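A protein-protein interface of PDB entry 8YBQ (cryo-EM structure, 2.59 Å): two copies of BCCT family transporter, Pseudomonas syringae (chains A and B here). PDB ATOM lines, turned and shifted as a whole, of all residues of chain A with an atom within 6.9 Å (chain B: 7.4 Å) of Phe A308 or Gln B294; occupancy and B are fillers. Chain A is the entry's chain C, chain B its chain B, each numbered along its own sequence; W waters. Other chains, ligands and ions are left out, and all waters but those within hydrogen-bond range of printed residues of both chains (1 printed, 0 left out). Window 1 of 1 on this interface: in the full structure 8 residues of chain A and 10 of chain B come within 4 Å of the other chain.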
ATOM      1  N   TRP A  60     -25.091  31.809 -17.126  1.00  0.00           N
ATOM      2  CA  TRP A  60     -23.901  31.194 -16.551  1.00  0.00           C
ATOM      3  C   TRP A  60     -24.167  30.539 -15.202  1.00  0.00           C
ATOM      4  O   TRP A  60     -23.523  29.535 -14.877  1.00  0.00           O
ATOM      5  CB  TRP A  60     -22.791  32.245 -16.405  1.00  0.00           C
ATOM      6  CG  TRP A  60     -23.216  33.436 -15.600  1.00  0.00           C
ATOM      7  CD1 TRP A  60     -23.914  34.513 -16.045  1.00  0.00           C
ATOM      8  CD2 TRP A  60     -22.987  33.657 -14.204  1.00  0.00           C
ATOM      9  NE1 TRP A  60     -24.136  35.392 -15.020  1.00  0.00           N
ATOM     10  CE2 TRP A  60     -23.578  34.889 -13.877  1.00  0.00           C
ATOM     11  CE3 TRP A  60     -22.342  32.931 -13.199  1.00  0.00           C
ATOM     12  CZ2 TRP A  60     -23.541  35.413 -12.591  1.00  0.00           C
ATOM     13  CZ3 TRP A  60     -22.309  33.453 -11.925  1.00  0.00           C
ATOM     14  CH2 TRP A  60     -22.902  34.681 -11.631  1.00  0.00           C
ATOM     15  N   MET A  63     -25.655  26.920 -15.687  1.00  0.00           N
ATOM     16  CA  MET A  63     -24.604  26.013 -16.133  1.00  0.00           C
ATOM     17  C   MET A  63     -23.609  25.725 -15.021  1.00  0.00           C
ATOM     18  O   MET A  63     -23.051  24.627 -14.960  1.00  0.00           O
ATOM     19  CB  MET A  63     -23.869  26.594 -17.340  1.00  0.00           C
ATOM     20  CG  MET A  63     -24.765  27.165 -18.420  1.00  0.00           C
ATOM     21  SD  MET A  63     -25.676  25.941 -19.375  1.00  0.00           S
ATOM     22  CE  MET A  63     -24.339  25.097 -20.202  1.00  0.00           C
ATOM     23  N   MET A  64     -23.370  26.692 -14.137  1.00  0.00           N
ATOM     24  CA  MET A  64     -22.439  26.456 -13.044  1.00  0.00           C
ATOM     25  C   MET A  64     -23.034  25.536 -11.982  1.00  0.00           C
ATOM     26  O   MET A  64     -22.329  24.677 -11.447  1.00  0.00           O
ATOM     27  CB  MET A  64     -22.013  27.786 -12.426  1.00  0.00           C
ATOM     28  CG  MET A  64     -20.586  27.799 -11.914  1.00  0.00           C
ATOM     29  SD  MET A  64     -19.374  27.503 -13.209  1.00  0.00           S
ATOM     30  CE  MET A  64     -17.970  26.958 -12.243  1.00  0.00           C
ATOM     31  N   THR A  67     -23.720  21.341 -12.744  1.00  0.00           N
ATOM     32  CA  THR A  67     -22.601  20.404 -12.733  1.00  0.00           C
ATOM     33  C   THR A  67     -22.193  20.015 -11.315  1.00  0.00           C
ATOM     34  O   THR A  67     -21.674  18.910 -11.098  1.00  0.00           O
ATOM     35  CB  THR A  67     -21.417  21.020 -13.477  1.00  0.00           C
ATOM     36  OG1 THR A  67     -21.830  21.384 -14.797  1.00  0.00           O
ATOM     37  CG2 THR A  67     -20.277  20.033 -13.595  1.00  0.00           C
ATOM     38  N   LEU A 303     -18.445  15.279 -23.379  1.00  0.00           N
ATOM     39  CA  LEU A 303     -19.086  15.634 -22.112  1.00  0.00           C
ATOM     40  C   LEU A 303     -18.330  16.661 -21.269  1.00  0.00           C
ATOM     41  O   LEU A 303     -18.959  17.638 -20.829  1.00  0.00           O
ATOM     42  CB  LEU A 303     -19.350  14.357 -21.306  1.00  0.00           C
ATOM     43  CG  LEU A 303     -20.253  14.439 -20.076  1.00  0.00           C
ATOM     44  CD1 LEU A 303     -21.498  15.260 -20.344  1.00  0.00           C
ATOM     45  CD2 LEU A 303     -20.622  13.045 -19.627  1.00  0.00           C
ATOM     46  N   PRO A 304     -17.030  16.514 -20.980  1.00  0.00           N
ATOM     47  CA  PRO A 304     -16.406  17.404 -19.984  1.00  0.00           C
ATOM     48  C   PRO A 304     -16.212  18.843 -20.442  1.00  0.00           C
ATOM     49  O   PRO A 304     -15.809  19.677 -19.622  1.00  0.00           O
ATOM     50  CB  PRO A 304     -15.055  16.729 -19.712  1.00  0.00           C
ATOM     51  CG  PRO A 304     -14.749  16.022 -20.958  1.00  0.00           C
ATOM     52  CD  PRO A 304     -16.062  15.525 -21.486  1.00  0.00           C
ATOM     53  N   SER A 305     -16.473  19.165 -21.708  1.00  0.00           N
ATOM     54  CA  SER A 305     -16.318  20.525 -22.197  1.00  0.00           C
ATOM     55  C   SER A 305     -17.631  21.183 -22.585  1.00  0.00           C
ATOM     56  O   SER A 305     -17.730  22.410 -22.514  1.00  0.00           O
ATOM     57  CB  SER A 305     -15.366  20.545 -23.402  1.00  0.00           C
ATOM     58  OG  SER A 305     -15.227  21.851 -23.935  1.00  0.00           O
ATOM     59  N   LYS A 306     -18.642  20.405 -22.972  1.00  0.00           N
ATOM     60  CA  LYS A 306     -19.954  20.934 -23.314  1.00  0.00           C
ATOM     61  C   LYS A 306     -20.769  21.327 -22.091  1.00  0.00           C
ATOM     62  O   LYS A 306     -21.867  21.869 -22.248  1.00  0.00           O
ATOM     63  CB  LYS A 306     -20.727  19.911 -24.145  1.00  0.00           C
ATOM     64  CG  LYS A 306     -20.749  20.214 -25.628  1.00  0.00           C
ATOM     65  CD  LYS A 306     -21.642  21.400 -25.917  1.00  0.00           C
ATOM     66  CE  LYS A 306     -21.503  21.881 -27.340  1.00  0.00           C
ATOM     67  NZ  LYS A 306     -22.383  23.050 -27.573  1.00  0.00           N
ATOM     68  N   SER A 307     -20.264  21.069 -20.888  1.00  0.00           N
ATOM     69  CA  SER A 307     -20.930  21.445 -19.651  1.00  0.00           C
ATOM     70  C   SER A 307     -20.843  22.937 -19.360  1.00  0.00           C
ATOM     71  O   SER A 307     -21.640  23.443 -18.568  1.00  0.00           O
ATOM     72  CB  SER A 307     -20.325  20.667 -18.482  1.00  0.00           C
ATOM     73  OG  SER A 307     -20.497  19.275 -18.653  1.00  0.00           O
ATOM     74  N   PHE A 308     -19.901  23.651 -19.980  1.00  0.00           N
ATOM     75  CA  PHE A 308     -19.730  25.072 -19.717  1.00  0.00           C
ATOM     76  C   PHE A 308     -19.861  25.926 -20.973  1.00  0.00           C
ATOM     77  O   PHE A 308     -19.466  27.096 -20.946  1.00  0.00           O
ATOM     78  CB  PHE A 308     -18.368  25.335 -19.062  1.00  0.00           C
ATOM     79  CG  PHE A 308     -18.156  24.595 -17.771  1.00  0.00           C
ATOM     80  CD1 PHE A 308     -18.686  25.072 -16.587  1.00  0.00           C
ATOM     81  CD2 PHE A 308     -17.419  23.426 -17.744  1.00  0.00           C
ATOM     82  CE1 PHE A 308     -18.490  24.393 -15.404  1.00  0.00           C
ATOM     83  CE2 PHE A 308     -17.219  22.743 -16.562  1.00  0.00           C
ATOM     84  CZ  PHE A 308     -17.754  23.229 -15.391  1.00  0.00           C
ATOM     85  N   ASP A 309     -20.405  25.392 -22.063  1.00  0.00           N
ATOM     86  CA  ASP A 309     -20.462  26.113 -23.328  1.00  0.00           C
ATOM     87  C   ASP A 309     -21.639  27.082 -23.335  1.00  0.00           C
ATOM     88  O   ASP A 309     -22.795  26.666 -23.218  1.00  0.00           O
ATOM     89  CB  ASP A 309     -20.572  25.134 -24.492  1.00  0.00           C
ATOM     90  CG  ASP A 309     -20.043  25.707 -25.787  1.00  0.00           C
ATOM     91  OD1 ASP A 309     -19.907  26.941 -25.888  1.00  0.00           O
ATOM     92  OD2 ASP A 309     -19.759  24.921 -26.711  1.00  0.00           O
ATOM     93  N   VAL A 310     -21.341  28.372 -23.486  1.00  0.00           N
ATOM     94  CA  VAL A 310     -22.351  29.416 -23.585  1.00  0.00           C
ATOM     95  C   VAL A 310     -22.222  30.237 -24.858  1.00  0.00           C
ATOM     96  O   VAL A 310     -22.929  31.237 -25.006  1.00  0.00           O
ATOM     97  CB  VAL A 310     -22.332  30.339 -22.350  1.00  0.00           C
ATOM     98  CG1 VAL A 310     -22.768  29.582 -21.113  1.00  0.00           C
ATOM     99  CG2 VAL A 310     -20.951  30.915 -22.139  1.00  0.00           C
ATOM    100  N   TYR A 311     -21.340  29.845 -25.781  1.00  0.00           N
ATOM    101  CA  TYR A 311     -21.165  30.504 -27.078  1.00  0.00           C
ATOM    102  C   TYR A 311     -20.835  31.989 -26.902  1.00  0.00           C
ATOM    103  O   TYR A 311     -21.451  32.869 -27.503  1.00  0.00           O
ATOM    104  CB  TYR A 311     -22.403  30.307 -27.962  1.00  0.00           C
ATOM    105  CG  TYR A 311     -22.909  28.883 -27.993  1.00  0.00           C
ATOM    106  CD1 TYR A 311     -22.372  27.956 -28.869  1.00  0.00           C
ATOM    107  CD2 TYR A 311     -23.920  28.466 -27.139  1.00  0.00           C
ATOM    108  CE1 TYR A 311     -22.825  26.655 -28.890  1.00  0.00           C
ATOM    109  CE2 TYR A 311     -24.376  27.171 -27.154  1.00  0.00           C
ATOM    110  CZ  TYR A 311     -23.828  26.271 -28.031  1.00  0.00           C
ATOM    111  OH  TYR A 311     -24.285  24.977 -28.048  1.00  0.00           O
ATOM    112  N   ALA A 312     -19.820  32.247 -26.078  1.00  0.00           N
ATOM    113  CA  ALA A 312     -19.513  33.596 -25.620  1.00  0.00           C
ATOM    114  C   ALA A 312     -18.706  34.419 -26.615  1.00  0.00           C
ATOM    115  O   ALA A 312     -18.744  35.651 -26.545  1.00  0.00           O
ATOM    116  CB  ALA A 312     -18.758  33.538 -24.291  1.00  0.00           C
ATOM    117  N   TYR A 313     -17.977  33.785 -27.527  1.00  0.00           N
ATOM    118  CA  TYR A 313     -17.187  34.503 -28.515  1.00  0.00           C
ATOM    119  C   TYR A 313     -17.899  34.648 -29.853  1.00  0.00           C
ATOM    120  O   TYR A 313     -17.317  35.196 -30.792  1.00  0.00           O
ATOM    121  CB  TYR A 313     -15.835  33.812 -28.715  1.00  0.00           C
ATOM    122  CG  TYR A 313     -14.917  33.931 -27.520  1.00  0.00           C
ATOM    123  CD1 TYR A 313     -14.312  35.138 -27.200  1.00  0.00           C
ATOM    124  CD2 TYR A 313     -14.664  32.840 -26.705  1.00  0.00           C
ATOM    125  CE1 TYR A 313     -13.481  35.250 -26.107  1.00  0.00           C
ATOM    126  CE2 TYR A 313     -13.835  32.945 -25.613  1.00  0.00           C
ATOM    127  CZ  TYR A 313     -13.247  34.149 -25.320  1.00  0.00           C
ATOM    128  OH  TYR A 313     -12.421  34.252 -24.230  1.00  0.00           O
ATOM    129  N   ARG B 140     -10.110  32.747 -28.367  1.00  0.00           N
ATOM    130  CA  ARG B 140     -10.439  31.564 -27.588  1.00  0.00           C
ATOM    131  C   ARG B 140      -9.207  30.713 -27.307  1.00  0.00           C
ATOM    132  O   ARG B 140      -9.123  30.083 -26.249  1.00  0.00           O
ATOM    133  CB  ARG B 140     -11.498  30.755 -28.333  1.00  0.00           C
ATOM    134  CG  ARG B 140     -12.331  29.824 -27.484  1.00  0.00           C
ATOM    135  CD  ARG B 140     -13.366  29.139 -28.348  1.00  0.00           C
ATOM    136  NE  ARG B 140     -14.127  28.124 -27.630  1.00  0.00           N
ATOM    137  CZ  ARG B 140     -15.027  27.330 -28.201  1.00  0.00           C
ATOM    138  NH1 ARG B 140     -15.276  27.436 -29.496  1.00  0.00           N
ATOM    139  NH2 ARG B 140     -15.676  26.431 -27.479  1.00  0.00           N
ATOM    140  N   PHE B 147      -4.540  30.334 -19.445  1.00  0.00           N
ATOM    141  CA  PHE B 147      -4.925  29.472 -18.331  1.00  0.00           C
ATOM    142  C   PHE B 147      -3.947  28.324 -18.131  1.00  0.00           C
ATOM    143  O   PHE B 147      -3.719  27.902 -16.995  1.00  0.00           O
ATOM    144  CB  PHE B 147      -6.330  28.905 -18.542  1.00  0.00           C
ATOM    145  CG  PHE B 147      -7.417  29.697 -17.873  1.00  0.00           C
ATOM    146  CD1 PHE B 147      -7.334  31.073 -17.773  1.00  0.00           C
ATOM    147  CD2 PHE B 147      -8.514  29.060 -17.331  1.00  0.00           C
ATOM    148  CE1 PHE B 147      -8.332  31.793 -17.160  1.00  0.00           C
ATOM    149  CE2 PHE B 147      -9.513  29.779 -16.714  1.00  0.00           C
ATOM    150  CZ  PHE B 147      -9.421  31.146 -16.630  1.00  0.00           C
ATOM    151  N   LEU B 288     -18.261  39.571 -19.243  1.00  0.00           N
ATOM    152  CA  LEU B 288     -17.131  39.051 -18.483  1.00  0.00           C
ATOM    153  C   LEU B 288     -17.510  37.795 -17.709  1.00  0.00           C
ATOM    154  O   LEU B 288     -16.728  36.836 -17.648  1.00  0.00           O
ATOM    155  CB  LEU B 288     -16.598  40.133 -17.546  1.00  0.00           C
ATOM    156  CG  LEU B 288     -15.903  41.310 -18.234  1.00  0.00           C
ATOM    157  CD1 LEU B 288     -15.516  42.373 -17.232  1.00  0.00           C
ATOM    158  CD2 LEU B 288     -14.692  40.838 -19.008  1.00  0.00           C
ATOM    159  N   LEU B 289     -18.713  37.767 -17.133  1.00  0.00           N
ATOM    160  CA  LEU B 289     -19.157  36.568 -16.429  1.00  0.00           C
ATOM    161  C   LEU B 289     -19.316  35.383 -17.374  1.00  0.00           C
ATOM    162  O   LEU B 289     -18.899  34.260 -17.047  1.00  0.00           O
ATOM    163  CB  LEU B 289     -20.463  36.854 -15.693  1.00  0.00           C
ATOM    164  CG  LEU B 289     -20.330  37.740 -14.454  1.00  0.00           C
ATOM    165  CD1 LEU B 289     -21.670  38.304 -14.047  1.00  0.00           C
ATOM    166  CD2 LEU B 289     -19.707  36.971 -13.313  1.00  0.00           C
ATOM    167  N   ASN B 290     -19.889  35.614 -18.557  1.00  0.00           N
ATOM    168  CA  ASN B 290     -20.019  34.534 -19.531  1.00  0.00           C
ATOM    169  C   ASN B 290     -18.659  34.012 -19.986  1.00  0.00           C
ATOM    170  O   ASN B 290     -18.454  32.792 -20.066  1.00  0.00           O
ATOM    171  CB  ASN B 290     -20.837  35.008 -20.730  1.00  0.00           C
ATOM    172  CG  ASN B 290     -22.283  35.265 -20.383  1.00  0.00           C
ATOM    173  OD1 ASN B 290     -23.054  34.336 -20.158  1.00  0.00           O
ATOM    174  ND2 ASN B 290     -22.665  36.531 -20.343  1.00  0.00           N
ATOM    175  N   THR B 291     -17.719  34.912 -20.285  1.00  0.00           N
ATOM    176  CA  THR B 291     -16.405  34.466 -20.738  1.00  0.00           C
ATOM    177  C   THR B 291     -15.634  33.745 -19.639  1.00  0.00           C
ATOM    178  O   THR B 291     -14.826  32.863 -19.943  1.00  0.00           O
ATOM    179  CB  THR B 291     -15.593  35.642 -21.279  1.00  0.00           C
ATOM    180  OG1 THR B 291     -15.526  36.678 -20.295  1.00  0.00           O
ATOM    181  CG2 THR B 291     -16.207  36.183 -22.553  1.00  0.00           C
ATOM    182  N   LEU B 292     -15.872  34.078 -18.368  1.00  0.00           N
ATOM    183  CA  LEU B 292     -15.233  33.332 -17.285  1.00  0.00           C
ATOM    184  C   LEU B 292     -15.632  31.857 -17.312  1.00  0.00           C
ATOM    185  O   LEU B 292     -14.772  30.961 -17.282  1.00  0.00           O
ATOM    186  CB  LEU B 292     -15.590  33.970 -15.943  1.00  0.00           C
ATOM    187  CG  LEU B 292     -15.059  33.367 -14.640  1.00  0.00           C
ATOM    188  CD1 LEU B 292     -13.560  33.139 -14.688  1.00  0.00           C
ATOM    189  CD2 LEU B 292     -15.414  34.270 -13.479  1.00  0.00           C
ATOM    190  N   VAL B 293     -16.939  31.587 -17.369  1.00  0.00           N
ATOM    191  CA  VAL B 293     -17.401  30.200 -17.426  1.00  0.00           C
ATOM    192  C   VAL B 293     -16.906  29.506 -18.696  1.00  0.00           C
ATOM    193  O   VAL B 293     -16.485  28.334 -18.657  1.00  0.00           O
ATOM    194  CB  VAL B 293     -18.936  30.160 -17.306  1.00  0.00           C
ATOM    195  CG1 VAL B 293     -19.454  28.746 -17.428  1.00  0.00           C
ATOM    196  CG2 VAL B 293     -19.367  30.763 -15.985  1.00  0.00           C
ATOM    197  N   GLN B 294     -16.935  30.209 -19.833  1.00  0.00           N
ATOM    198  CA  GLN B 294     -16.420  29.642 -21.077  1.00  0.00           C
ATOM    199  C   GLN B 294     -14.956  29.227 -20.946  1.00  0.00           C
ATOM    200  O   GLN B 294     -14.569  28.143 -21.401  1.00  0.00           O
ATOM    201  CB  GLN B 294     -16.593  30.651 -22.210  1.00  0.00           C
ATOM    202  CG  GLN B 294     -16.150  30.156 -23.572  1.00  0.00           C
ATOM    203  CD  GLN B 294     -17.221  29.361 -24.276  1.00  0.00           C
ATOM    204  OE1 GLN B 294     -18.398  29.688 -24.197  1.00  0.00           O
ATOM    205  NE2 GLN B 294     -16.819  28.306 -24.962  1.00  0.00           N
ATOM    206  N   ASN B 295     -14.129  30.078 -20.332  1.00  0.00           N
ATOM    207  CA  ASN B 295     -12.709  29.775 -20.181  1.00  0.00           C
ATOM    208  C   ASN B 295     -12.482  28.569 -19.284  1.00  0.00           C
ATOM    209  O   ASN B 295     -11.621  27.730 -19.581  1.00  0.00           O
ATOM    210  CB  ASN B 295     -11.970  30.988 -19.618  1.00  0.00           C
ATOM    211  CG  ASN B 295     -11.836  32.110 -20.621  1.00  0.00           C
ATOM    212  OD1 ASN B 295     -11.924  31.897 -21.825  1.00  0.00           O
ATOM    213  ND2 ASN B 295     -11.620  33.315 -20.124  1.00  0.00           N
ATOM    214  N   ILE B 296     -13.221  28.478 -18.174  1.00  0.00           N
ATOM    215  CA  ILE B 296     -13.102  27.302 -17.308  1.00  0.00           C
ATOM    216  C   ILE B 296     -13.387  26.030 -18.099  1.00  0.00           C
ATOM    217  O   ILE B 296     -12.633  25.044 -18.036  1.00  0.00           O
ATOM    218  CB  ILE B 296     -14.039  27.427 -16.094  1.00  0.00           C
ATOM    219  CG1 ILE B 296     -13.558  28.522 -15.146  1.00  0.00           C
ATOM    220  CG2 ILE B 296     -14.141  26.102 -15.359  1.00  0.00           C
ATOM    221  CD1 ILE B 296     -14.554  28.856 -14.069  1.00  0.00           C
ATOM    222  N   GLY B 297     -14.483  26.037 -18.861  1.00  0.00           N
ATOM    223  CA  GLY B 297     -14.830  24.861 -19.645  1.00  0.00           C
ATOM    224  C   GLY B 297     -13.775  24.492 -20.670  1.00  0.00           C
ATOM    225  O   GLY B 297     -13.416  23.320 -20.807  1.00  0.00           O
ATOM    226  N   ASP B 298     -13.263  25.485 -21.403  1.00  0.00           N
ATOM    227  CA  ASP B 298     -12.253  25.216 -22.423  1.00  0.00           C
ATOM    228  C   ASP B 298     -10.975  24.642 -21.823  1.00  0.00           C
ATOM    229  O   ASP B 298     -10.411  23.680 -22.364  1.00  0.00           O
ATOM    230  CB  ASP B 298     -11.935  26.493 -23.195  1.00  0.00           C
ATOM    231  CG  ASP B 298     -13.017  26.863 -24.178  1.00  0.00           C
ATOM    232  OD1 ASP B 298     -13.691  25.953 -24.696  1.00  0.00           O
ATOM    233  OD2 ASP B 298     -13.189  28.070 -24.440  1.00  0.00           O
ATOM    234  N   TYR B 299     -10.501  25.218 -20.716  1.00  0.00           N
ATOM    235  CA  TYR B 299      -9.302  24.706 -20.062  1.00  0.00           C
ATOM    236  C   TYR B 299      -9.478  23.263 -19.610  1.00  0.00           C
ATOM    237  O   TYR B 299      -8.622  22.411 -19.893  1.00  0.00           O
ATOM    238  CB  TYR B 299      -8.942  25.593 -18.873  1.00  0.00           C
ATOM    239  CG  TYR B 299      -7.701  25.167 -18.126  1.00  0.00           C
ATOM    240  CD1 TYR B 299      -7.710  25.026 -16.748  1.00  0.00           C
ATOM    241  CD2 TYR B 299      -6.516  24.915 -18.800  1.00  0.00           C
ATOM    242  CE1 TYR B 299      -6.579  24.643 -16.064  1.00  0.00           C
ATOM    243  CE2 TYR B 299      -5.383  24.529 -18.124  1.00  0.00           C
ATOM    244  CZ  TYR B 299      -5.419  24.397 -16.757  1.00  0.00           C
ATOM    245  OH  TYR B 299      -4.288  24.014 -16.082  1.00  0.00           O
ATOM    246  N   LEU B 300     -10.567  22.965 -18.892  1.00  0.00           N
ATOM    247  CA  LEU B 300     -10.742  21.598 -18.411  1.00  0.00           C
ATOM    248  C   LEU B 300     -10.942  20.619 -19.558  1.00  0.00           C
ATOM    249  O   LEU B 300     -10.540  19.455 -19.449  1.00  0.00           O
ATOM    250  CB  LEU B 300     -11.910  21.517 -17.433  1.00  0.00           C
ATOM    251  CG  LEU B 300     -11.597  22.016 -16.024  1.00  0.00           C
ATOM    252  CD1 LEU B 300     -12.743  21.706 -15.082  1.00  0.00           C
ATOM    253  CD2 LEU B 300     -10.301  21.414 -15.519  1.00  0.00           C
ATOM    254  N   GLY B 301     -11.543  21.059 -20.665  1.00  0.00           N
ATOM    255  CA  GLY B 301     -11.705  20.173 -21.800  1.00  0.00           C
ATOM    256  C   GLY B 301     -10.428  19.848 -22.540  1.00  0.00           C
ATOM    257  O   GLY B 301     -10.285  18.726 -23.032  1.00  0.00           O
HETATM  258  O   HOH W   1     -16.626  25.341 -23.130  1.00  0.00           O
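The side-chain amide oxygen (OE1) of Gln B294 is in hydrogen-bond range of the backbone NH (N) of Val A310, at 3.3 Å. The backbone NH of Tyr A311 sits at hydrogen-bond distance from the side-chain amide oxygen of Gln B294, at 3.3 Å. The backbone NH of Ala A312 is in hydrogen-bond range of the side-chain amide oxygen of Gln B294 (3.5 Å). The side-chain amide oxygen (OD1) of Asn B295 is in hydrogen-bond range of the side-chain hydroxyl (OH) of Tyr A313.
NE2 of Gln B294 sits close to NH2 of Arg B140, at 3.3 Å. The side-chain carboxylate (OD2) of Asp B298 lies within salt-bridge range of the guanidinium group (NE) of Arg B140, at 3.3 Å. The backbone carbonyl oxygen (O) of Thr B291 lies close to the side-chain amide nitrogen (ND2) of Asn B295 (3.2 Å). NZ of Lys A306 is in salt-bridge range of OD2 of Asp A309, at 3.3 Å. The side-chain amino group of Lys A306 is in hydrogen-bond range of the side-chain hydroxyl of Tyr A311, at 2.7 Å. The side-chain carboxylate (OD1) of Asp A309 sits at hydrogen-bond distance from the backbone NH (N) of Tyr A311 (3.2 Å).
Trp A60 touches Leu B289. Trp A60 touches Val B293 (CB to CG2, 3.8 Å). Gly B297 touches Ser A305 (O to OG, 3.9 Å). CB of Phe A308 touches O of Val B293 (3.6 Å). O of Phe A308 touches CA of Gln B294, at 3.97 Å. Phe A308 touches Gly B297. Gln B294 touches Asp A309. Val A310 touches Asn B290 (CG2 to O, 3.7 Å). Tyr A313 touches Arg B140.
Of the printed residues of chain B, Trp A60 touches Leu B289 (3.7 Å) and Val B293 (3.8 Å). Of chain B, only Val B293 (3.6 Å), Gln B294 (3.97 Å) and Gly B297 (3.5 Å) come within 4 Å of Phe A308. Of the printed residues of chain B, Asp A309 touches Gln B294. Printed residues of chain B within 4 Å of Ala A312: Gln B294. Phe B147 touches none of the printed residues of chain A. Of the printed residues of chain A, Leu B289 touches Trp A60. Of chain A, only Phe A308 (3.97 Å), Asp A309 (3.5 Å), Val A310 (3.3 Å), Tyr A311 (3.3 Å) and Ala A312 (3.5 Å) come within 4 Å of Gln B294. Printed residues of chain A within 4 Å of Gly B297: Ser A305 and Phe A308. The nearest residue of chain B that does not touch Phe A308 is Ile B296 (4.6 Å).
Printed residues of chain B that touch a printed residue of chain A: Arg B140, Leu B289, Asn B290, Val B293, Gln B294, Asn B295 and Gly B297. Hydrophobic or aromatic side chains of chain B that line the printed part of chain A: Leu B289 and Val B293. Hydrophobic or aromatic side chains of chain A that line the printed part of chain B: Trp A60, Phe A308, Val A310, Ala A312 and Tyr A313. Among the printed residues, no Asp or Glu carboxylate lies within 4 Å of a Lys or Arg side-chain nitrogen of the other chain.
No position is printed for both chains.
Water W1 lies within hydrogen-bond range of the backbone carbonyl oxygen (O) of Ser A305 (3.2 Å), the side-chain carboxylate (OD1) of Asp B298 (3.4 Å) and the side-chain amide nitrogen (NE2) of Gln B294 (3.5 Å).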
